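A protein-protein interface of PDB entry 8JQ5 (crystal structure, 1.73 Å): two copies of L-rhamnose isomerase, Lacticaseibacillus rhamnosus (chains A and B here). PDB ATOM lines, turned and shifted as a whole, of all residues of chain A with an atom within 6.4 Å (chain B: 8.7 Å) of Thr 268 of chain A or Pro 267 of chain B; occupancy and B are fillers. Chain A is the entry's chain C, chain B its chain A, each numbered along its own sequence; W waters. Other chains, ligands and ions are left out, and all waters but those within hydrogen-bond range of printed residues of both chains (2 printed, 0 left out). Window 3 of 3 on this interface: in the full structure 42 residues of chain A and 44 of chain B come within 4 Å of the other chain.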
ATOM      1  N   HIS A 266      28.694  15.451  -1.793  1.00  0.00           N
ATOM      2  CA  HIS A 266      28.831  15.536  -0.322  1.00  0.00           C
ATOM      3  C   HIS A 266      27.770  14.673   0.337  1.00  0.00           C
ATOM      4  O   HIS A 266      26.721  14.394  -0.235  1.00  0.00           O
ATOM      5  CB  HIS A 266      28.704  16.990   0.142  1.00  0.00           C
ATOM      6  CG  HIS A 266      29.889  17.822  -0.210  1.00  0.00           C
ATOM      7  ND1 HIS A 266      29.972  18.508  -1.401  1.00  0.00           N
ATOM      8  CD2 HIS A 266      31.028  18.076   0.471  1.00  0.00           C
ATOM      9  CE1 HIS A 266      31.125  19.159  -1.446  1.00  0.00           C
ATOM     10  NE2 HIS A 266      31.795  18.905  -0.295  1.00  0.00           N
ATOM     11  N   PRO A 267      28.004  14.238   1.584  1.00  0.00           N
ATOM     12  CA  PRO A 267      26.919  13.653   2.363  1.00  0.00           C
ATOM     13  C   PRO A 267      25.717  14.615   2.391  1.00  0.00           C
ATOM     14  O   PRO A 267      25.924  15.814   2.599  1.00  0.00           O
ATOM     15  CB  PRO A 267      27.510  13.457   3.762  1.00  0.00           C
ATOM     16  CG  PRO A 267      29.023  13.633   3.609  1.00  0.00           C
ATOM     17  CD  PRO A 267      29.295  14.297   2.280  1.00  0.00           C
ATOM     18  N   THR A 268      24.512  14.077   2.160  1.00  0.00           N
ATOM     19  CA  THR A 268      23.196  14.776   2.157  1.00  0.00           C
ATOM     20  C   THR A 268      22.997  15.584   0.867  1.00  0.00           C
ATOM     21  O   THR A 268      21.905  16.143   0.691  1.00  0.00           O
ATOM     22  CB  THR A 268      23.007  15.666   3.390  1.00  0.00           C
ATOM     23  OG1 THR A 268      23.735  16.890   3.233  1.00  0.00           O
ATOM     24  CG2 THR A 268      23.432  14.969   4.663  1.00  0.00           C
ATOM     25  N   GLU A 269      23.983  15.647  -0.016  1.00  0.00           N
ATOM     26  CA  GLU A 269      23.868  16.497  -1.231  1.00  0.00           C
ATOM     27  C   GLU A 269      22.839  15.864  -2.161  1.00  0.00           C
ATOM     28  O   GLU A 269      22.918  14.654  -2.386  1.00  0.00           O
ATOM     29  CB  GLU A 269      25.217  16.686  -1.918  1.00  0.00           C
ATOM     30  CG  GLU A 269      25.201  17.748  -3.003  1.00  0.00           C
ATOM     31  CD  GLU A 269      26.538  18.450  -3.162  1.00  0.00           C
ATOM     32  OE1 GLU A 269      27.551  17.902  -2.657  1.00  0.00           O
ATOM     33  OE2 GLU A 269      26.566  19.548  -3.753  1.00  0.00           O
ATOM     34  N   ASP A 270      21.894  16.672  -2.638  1.00  0.00           N
ATOM     35  CA  ASP A 270      20.801  16.263  -3.552  1.00  0.00           C
ATOM     36  C   ASP A 270      21.148  16.761  -4.961  1.00  0.00           C
ATOM     37  O   ASP A 270      20.958  17.961  -5.254  1.00  0.00           O
ATOM     38  CB  ASP A 270      19.464  16.792  -3.042  1.00  0.00           C
ATOM     39  CG  ASP A 270      18.297  16.443  -3.945  1.00  0.00           C
ATOM     40  OD1 ASP A 270      18.535  15.758  -4.967  1.00  0.00           O
ATOM     41  OD2 ASP A 270      17.160  16.853  -3.611  1.00  0.00           O
ATOM     42  N   ARG A 309      14.162  11.505  -6.674  1.00  0.00           N
ATOM     43  CA  ARG A 309      14.343  12.974  -6.782  1.00  0.00           C
ATOM     44  C   ARG A 309      14.970  13.315  -8.130  1.00  0.00           C
ATOM     45  O   ARG A 309      14.457  14.251  -8.792  1.00  0.00           O
ATOM     46  CB  ARG A 309      15.152  13.503  -5.603  1.00  0.00           C
ATOM     47  CG  ARG A 309      14.321  13.621  -4.335  1.00  0.00           C
ATOM     48  CD  ARG A 309      15.210  13.884  -3.140  1.00  0.00           C
ATOM     49  NE  ARG A 309      14.420  14.011  -1.925  1.00  0.00           N
ATOM     50  CZ  ARG A 309      14.923  14.211  -0.723  1.00  0.00           C
ATOM     51  NH1 ARG A 309      16.230  14.283  -0.561  1.00  0.00           N
ATOM     52  NH2 ARG A 309      14.117  14.326   0.315  1.00  0.00           N
ATOM     53  N   LEU B 231      22.403  27.026   1.088  1.00  0.00           N
ATOM     54  CA  LEU B 231      21.863  25.664   0.863  1.00  0.00           C
ATOM     55  C   LEU B 231      20.464  25.585   1.472  1.00  0.00           C
ATOM     56  O   LEU B 231      19.547  25.065   0.799  1.00  0.00           O
ATOM     57  CB  LEU B 231      22.802  24.625   1.474  1.00  0.00           C
ATOM     58  CG  LEU B 231      22.271  23.193   1.481  1.00  0.00           C
ATOM     59  CD1 LEU B 231      22.014  22.705   0.069  1.00  0.00           C
ATOM     60  CD2 LEU B 231      23.232  22.259   2.203  1.00  0.00           C
ATOM     61  N   PHE B 232      20.298  26.080   2.700  1.00  0.00           N
ATOM     62  CA  PHE B 232      19.006  26.017   3.425  1.00  0.00           C
ATOM     63  C   PHE B 232      18.982  27.005   4.589  1.00  0.00           C
ATOM     64  O   PHE B 232      20.043  27.386   5.113  1.00  0.00           O
ATOM     65  CB  PHE B 232      18.774  24.601   3.944  1.00  0.00           C
ATOM     66  CG  PHE B 232      19.543  24.257   5.188  1.00  0.00           C
ATOM     67  CD1 PHE B 232      20.888  23.935   5.116  1.00  0.00           C
ATOM     68  CD2 PHE B 232      18.921  24.241   6.428  1.00  0.00           C
ATOM     69  CE1 PHE B 232      21.601  23.605   6.262  1.00  0.00           C
ATOM     70  CE2 PHE B 232      19.633  23.907   7.570  1.00  0.00           C
ATOM     71  CZ  PHE B 232      20.973  23.596   7.485  1.00  0.00           C
ATOM     72  N   GLY B 263      29.192  29.451   6.166  1.00  0.00           N
ATOM     73  CA  GLY B 263      28.150  28.789   6.978  1.00  0.00           C
ATOM     74  C   GLY B 263      27.027  28.205   6.133  1.00  0.00           C
ATOM     75  O   GLY B 263      26.113  27.596   6.706  1.00  0.00           O
ATOM     76  N   HIS B 264      27.094  28.345   4.808  1.00  0.00           N
ATOM     77  CA  HIS B 264      25.923  28.161   3.909  1.00  0.00           C
ATOM     78  C   HIS B 264      26.038  26.896   3.042  1.00  0.00           C
ATOM     79  O   HIS B 264      25.250  26.776   2.067  1.00  0.00           O
ATOM     80  CB  HIS B 264      25.754  29.423   3.063  1.00  0.00           C
ATOM     81  CG  HIS B 264      25.235  30.602   3.818  1.00  0.00           C
ATOM     82  ND1 HIS B 264      24.769  31.732   3.166  1.00  0.00           N
ATOM     83  CD2 HIS B 264      25.083  30.834   5.141  1.00  0.00           C
ATOM     84  CE1 HIS B 264      24.375  32.614   4.061  1.00  0.00           C
ATOM     85  NE2 HIS B 264      24.545  32.088   5.280  1.00  0.00           N
ATOM     86  N   PHE B 265      26.945  25.972   3.366  1.00  0.00           N
ATOM     87  CA  PHE B 265      27.266  24.801   2.508  1.00  0.00           C
ATOM     88  C   PHE B 265      26.854  23.499   3.215  1.00  0.00           C
ATOM     89  O   PHE B 265      26.234  23.536   4.307  1.00  0.00           O
ATOM     90  CB  PHE B 265      28.729  24.891   2.051  1.00  0.00           C
ATOM     91  CG  PHE B 265      28.972  25.976   1.027  1.00  0.00           C
ATOM     92  CD1 PHE B 265      29.055  27.306   1.407  1.00  0.00           C
ATOM     93  CD2 PHE B 265      29.058  25.674  -0.325  1.00  0.00           C
ATOM     94  CE1 PHE B 265      29.265  28.303   0.469  1.00  0.00           C
ATOM     95  CE2 PHE B 265      29.248  26.677  -1.272  1.00  0.00           C
ATOM     96  CZ  PHE B 265      29.352  27.989  -0.872  1.00  0.00           C
ATOM     97  N   HIS B 266      27.144  22.366   2.573  1.00  0.00           N
ATOM     98  CA  HIS B 266      26.792  21.005   3.059  1.00  0.00           C
ATOM     99  C   HIS B 266      27.651  20.641   4.260  1.00  0.00           C
ATOM    100  O   HIS B 266      28.746  21.179   4.450  1.00  0.00           O
ATOM    101  CB  HIS B 266      26.987  19.967   1.952  1.00  0.00           C
ATOM    102  CG  HIS B 266      25.995  20.088   0.847  1.00  0.00           C
ATOM    103  ND1 HIS B 266      26.205  20.914  -0.241  1.00  0.00           N
ATOM    104  CD2 HIS B 266      24.800  19.490   0.660  1.00  0.00           C
ATOM    105  CE1 HIS B 266      25.159  20.838  -1.041  1.00  0.00           C
ATOM    106  NE2 HIS B 266      24.288  19.958  -0.511  1.00  0.00           N
ATOM    107  N   PRO B 267      27.183  19.686   5.092  1.00  0.00           N
ATOM    108  CA  PRO B 267      28.054  19.058   6.075  1.00  0.00           C
ATOM    109  C   PRO B 267      29.330  18.551   5.386  1.00  0.00           C
ATOM    110  O   PRO B 267      29.221  17.922   4.343  1.00  0.00           O
ATOM    111  CB  PRO B 267      27.246  17.883   6.649  1.00  0.00           C
ATOM    112  CG  PRO B 267      25.826  18.064   6.159  1.00  0.00           C
ATOM    113  CD  PRO B 267      25.828  19.117   5.068  1.00  0.00           C
ATOM    114  N   THR B 268      30.490  18.874   5.971  1.00  0.00           N
ATOM    115  CA  THR B 268      31.864  18.456   5.571  1.00  0.00           C
ATOM    116  C   THR B 268      32.340  19.230   4.343  1.00  0.00           C
ATOM    117  O   THR B 268      33.490  18.990   3.923  1.00  0.00           O
ATOM    118  CB  THR B 268      31.990  16.949   5.305  1.00  0.00           C
ATOM    119  OG1 THR B 268      31.428  16.622   4.034  1.00  0.00           O
ATOM    120  CG2 THR B 268      31.327  16.102   6.366  1.00  0.00           C
ATOM    121  N   GLU B 269      31.510  20.107   3.775  1.00  0.00           N
ATOM    122  CA  GLU B 269      31.892  20.856   2.551  1.00  0.00           C
ATOM    123  C   GLU B 269      32.976  21.879   2.921  1.00  0.00           C
ATOM    124  O   GLU B 269      32.832  22.577   3.933  1.00  0.00           O
ATOM    125  CB  GLU B 269      30.659  21.460   1.885  1.00  0.00           C
ATOM    126  CG  GLU B 269      30.962  22.100   0.531  1.00  0.00           C
ATOM    127  CD  GLU B 269      29.763  22.165  -0.393  1.00  0.00           C
ATOM    128  OE1 GLU B 269      29.964  22.317  -1.585  1.00  0.00           O
ATOM    129  OE2 GLU B 269      28.633  22.076   0.098  1.00  0.00           O
ATOM    130  N   ASP B 270      34.058  21.903   2.144  1.00  0.00           N
ATOM    131  CA  ASP B 270      35.237  22.783   2.343  1.00  0.00           C
ATOM    132  C   ASP B 270      35.156  23.917   1.334  1.00  0.00           C
ATOM    133  O   ASP B 270      35.525  23.675   0.184  1.00  0.00           O
ATOM    134  CB  ASP B 270      36.539  22.014   2.128  1.00  0.00           C
ATOM    135  CG  ASP B 270      37.796  22.814   2.426  1.00  0.00           C
ATOM    136  OD1 ASP B 270      37.682  24.058   2.634  1.00  0.00           O
ATOM    137  OD2 ASP B 270      38.880  22.188   2.438  1.00  0.00           O
ATOM    138  N   PRO B 292      29.352  27.892  11.054  1.00  0.00           N
ATOM    139  CA  PRO B 292      28.139  27.093  11.207  1.00  0.00           C
ATOM    140  C   PRO B 292      28.380  25.986  12.241  1.00  0.00           C
ATOM    141  O   PRO B 292      29.399  25.321  12.180  1.00  0.00           O
ATOM    142  CB  PRO B 292      27.960  26.507   9.804  1.00  0.00           C
ATOM    143  CG  PRO B 292      29.379  26.267   9.351  1.00  0.00           C
ATOM    144  CD  PRO B 292      30.171  27.433   9.921  1.00  0.00           C
ATOM    145  N   ARG B 294      26.313  22.969  12.785  1.00  0.00           N
ATOM    146  CA  ARG B 294      25.324  21.947  12.344  1.00  0.00           C
ATOM    147  C   ARG B 294      24.165  22.579  11.567  1.00  0.00           C
ATOM    148  O   ARG B 294      23.329  21.816  11.047  1.00  0.00           O
ATOM    149  CB  ARG B 294      24.835  21.149  13.548  1.00  0.00           C
ATOM    150  CG  ARG B 294      25.985  20.526  14.321  1.00  0.00           C
ATOM    151  CD  ARG B 294      25.575  19.332  15.146  1.00  0.00           C
ATOM    152  NE  ARG B 294      26.762  18.702  15.687  1.00  0.00           N
ATOM    153  CZ  ARG B 294      27.496  17.809  15.033  1.00  0.00           C
ATOM    154  NH1 ARG B 294      27.144  17.427  13.817  1.00  0.00           N
ATOM    155  NH2 ARG B 294      28.571  17.291  15.599  1.00  0.00           N
ATOM    156  N   TRP B 295      24.132  23.908  11.472  1.00  0.00           N
ATOM    157  CA  TRP B 295      23.218  24.667  10.580  1.00  0.00           C
ATOM    158  C   TRP B 295      23.831  26.050  10.347  1.00  0.00           C
ATOM    159  O   TRP B 295      24.923  26.303  10.897  1.00  0.00           O
ATOM    160  CB  TRP B 295      21.788  24.704  11.155  1.00  0.00           C
ATOM    161  CG  TRP B 295      21.557  25.613  12.328  1.00  0.00           C
ATOM    162  CD1 TRP B 295      21.938  25.403  13.619  1.00  0.00           C
ATOM    163  CD2 TRP B 295      20.830  26.859  12.330  1.00  0.00           C
ATOM    164  NE1 TRP B 295      21.523  26.437  14.414  1.00  0.00           N
ATOM    165  CE2 TRP B 295      20.844  27.349  13.655  1.00  0.00           C
ATOM    166  CE3 TRP B 295      20.198  27.622  11.343  1.00  0.00           C
ATOM    167  CZ2 TRP B 295      20.246  28.558  14.018  1.00  0.00           C
ATOM    168  CZ3 TRP B 295      19.604  28.815  11.700  1.00  0.00           C
ATOM    169  CH2 TRP B 295      19.646  29.284  13.012  1.00  0.00           C
HETATM  170  O   HOH W   1      21.993  19.561  -2.116  1.00  0.00           O
HETATM  171  O   HOH W   2      34.194  20.282  -0.217  1.00  0.00           O
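ND1 of His 266 of chain A sits at hydrogen-bond distance from OE1 of Glu 269 of chain A (2.8 Å). A ring nitrogen (ND1) of His 266 of chain B is in hydrogen-bond range of the side-chain carboxylate (OE2) of Glu 269 of chain B, at 2.7 Å.
Of the printed residues of chain B, His 266 of chain A touches His 266, Thr 268 and Glu 269. Pro 267 of chain A touches one residue of chain B. Of chain B, only His 266 and Pro 267 come within 4 Å of Thr 268 of chain A. Asp 270 of chain A touches none of the printed residues of chain B. Leu 231 of chain B touches none of the printed residues of chain A. Of the printed residues of chain A, Thr 268 of chain B touches His 266 (3.9 Å) and Pro 267 (3.6 Å). The nearest residue of chain A that does not touch Pro 267 of chain B is Pro 267 of chain A (4.1 Å).
His 266 of chain A touches its own counterpart, His 266 of chain B. His 266 of chain A touches Thr 268 of chain B, and with the chains exchanged Thr 268 of chain A touches His 266 of chain B. His 266 of chain A touches Glu 269 of chain B, and with the chains exchanged Glu 269 of chain A touches His 266 of chain B. Pro 267 of chain A touches Thr 268 of chain B, and with the chains exchanged Thr 268 of chain A touches Pro 267 of chain B.
Water W2 lies within hydrogen-bond range of a ring nitrogen (NE2) of His 266 of chain A and the backbone NH (N) of Asp 270 of chain B. Water W1 lies within hydrogen-bond range of a ring nitrogen (NE2) of His 266 of chain B (2.8 Å) and the backbone NH of Asp 270 of chain A (2.9 Å).
Of the 13 printed residues of chain B, 4 touch a printed residue of chain A. Printed residues of chain A that touch a printed residue of chain B: His 266, Pro 267, Thr 268 and Glu 269. Among the printed residues, no Asp or Glu carboxylate lies within 4 Å of a Lys or Arg side-chain nitrogen of the other chain.
Among the printed residues, pairs that only touch across the chains: His 266 of chain A with His 266 of chain B (3.9 Å), His 266 of chain A with Thr 268 of chain B (3.9 Å), His 266 of chain A with Glu 269 of chain B (3.4 Å), Pro 267 of chain A with Thr 268 of chain B (3.6 Å), Thr 268 of chain A with His 266 of chain B (3.8 Å), Thr 268 of chain A with Pro 267 of chain B (3.6 Å) and Glu 269 of chain A with His 266 of chain B (3.3 Å).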
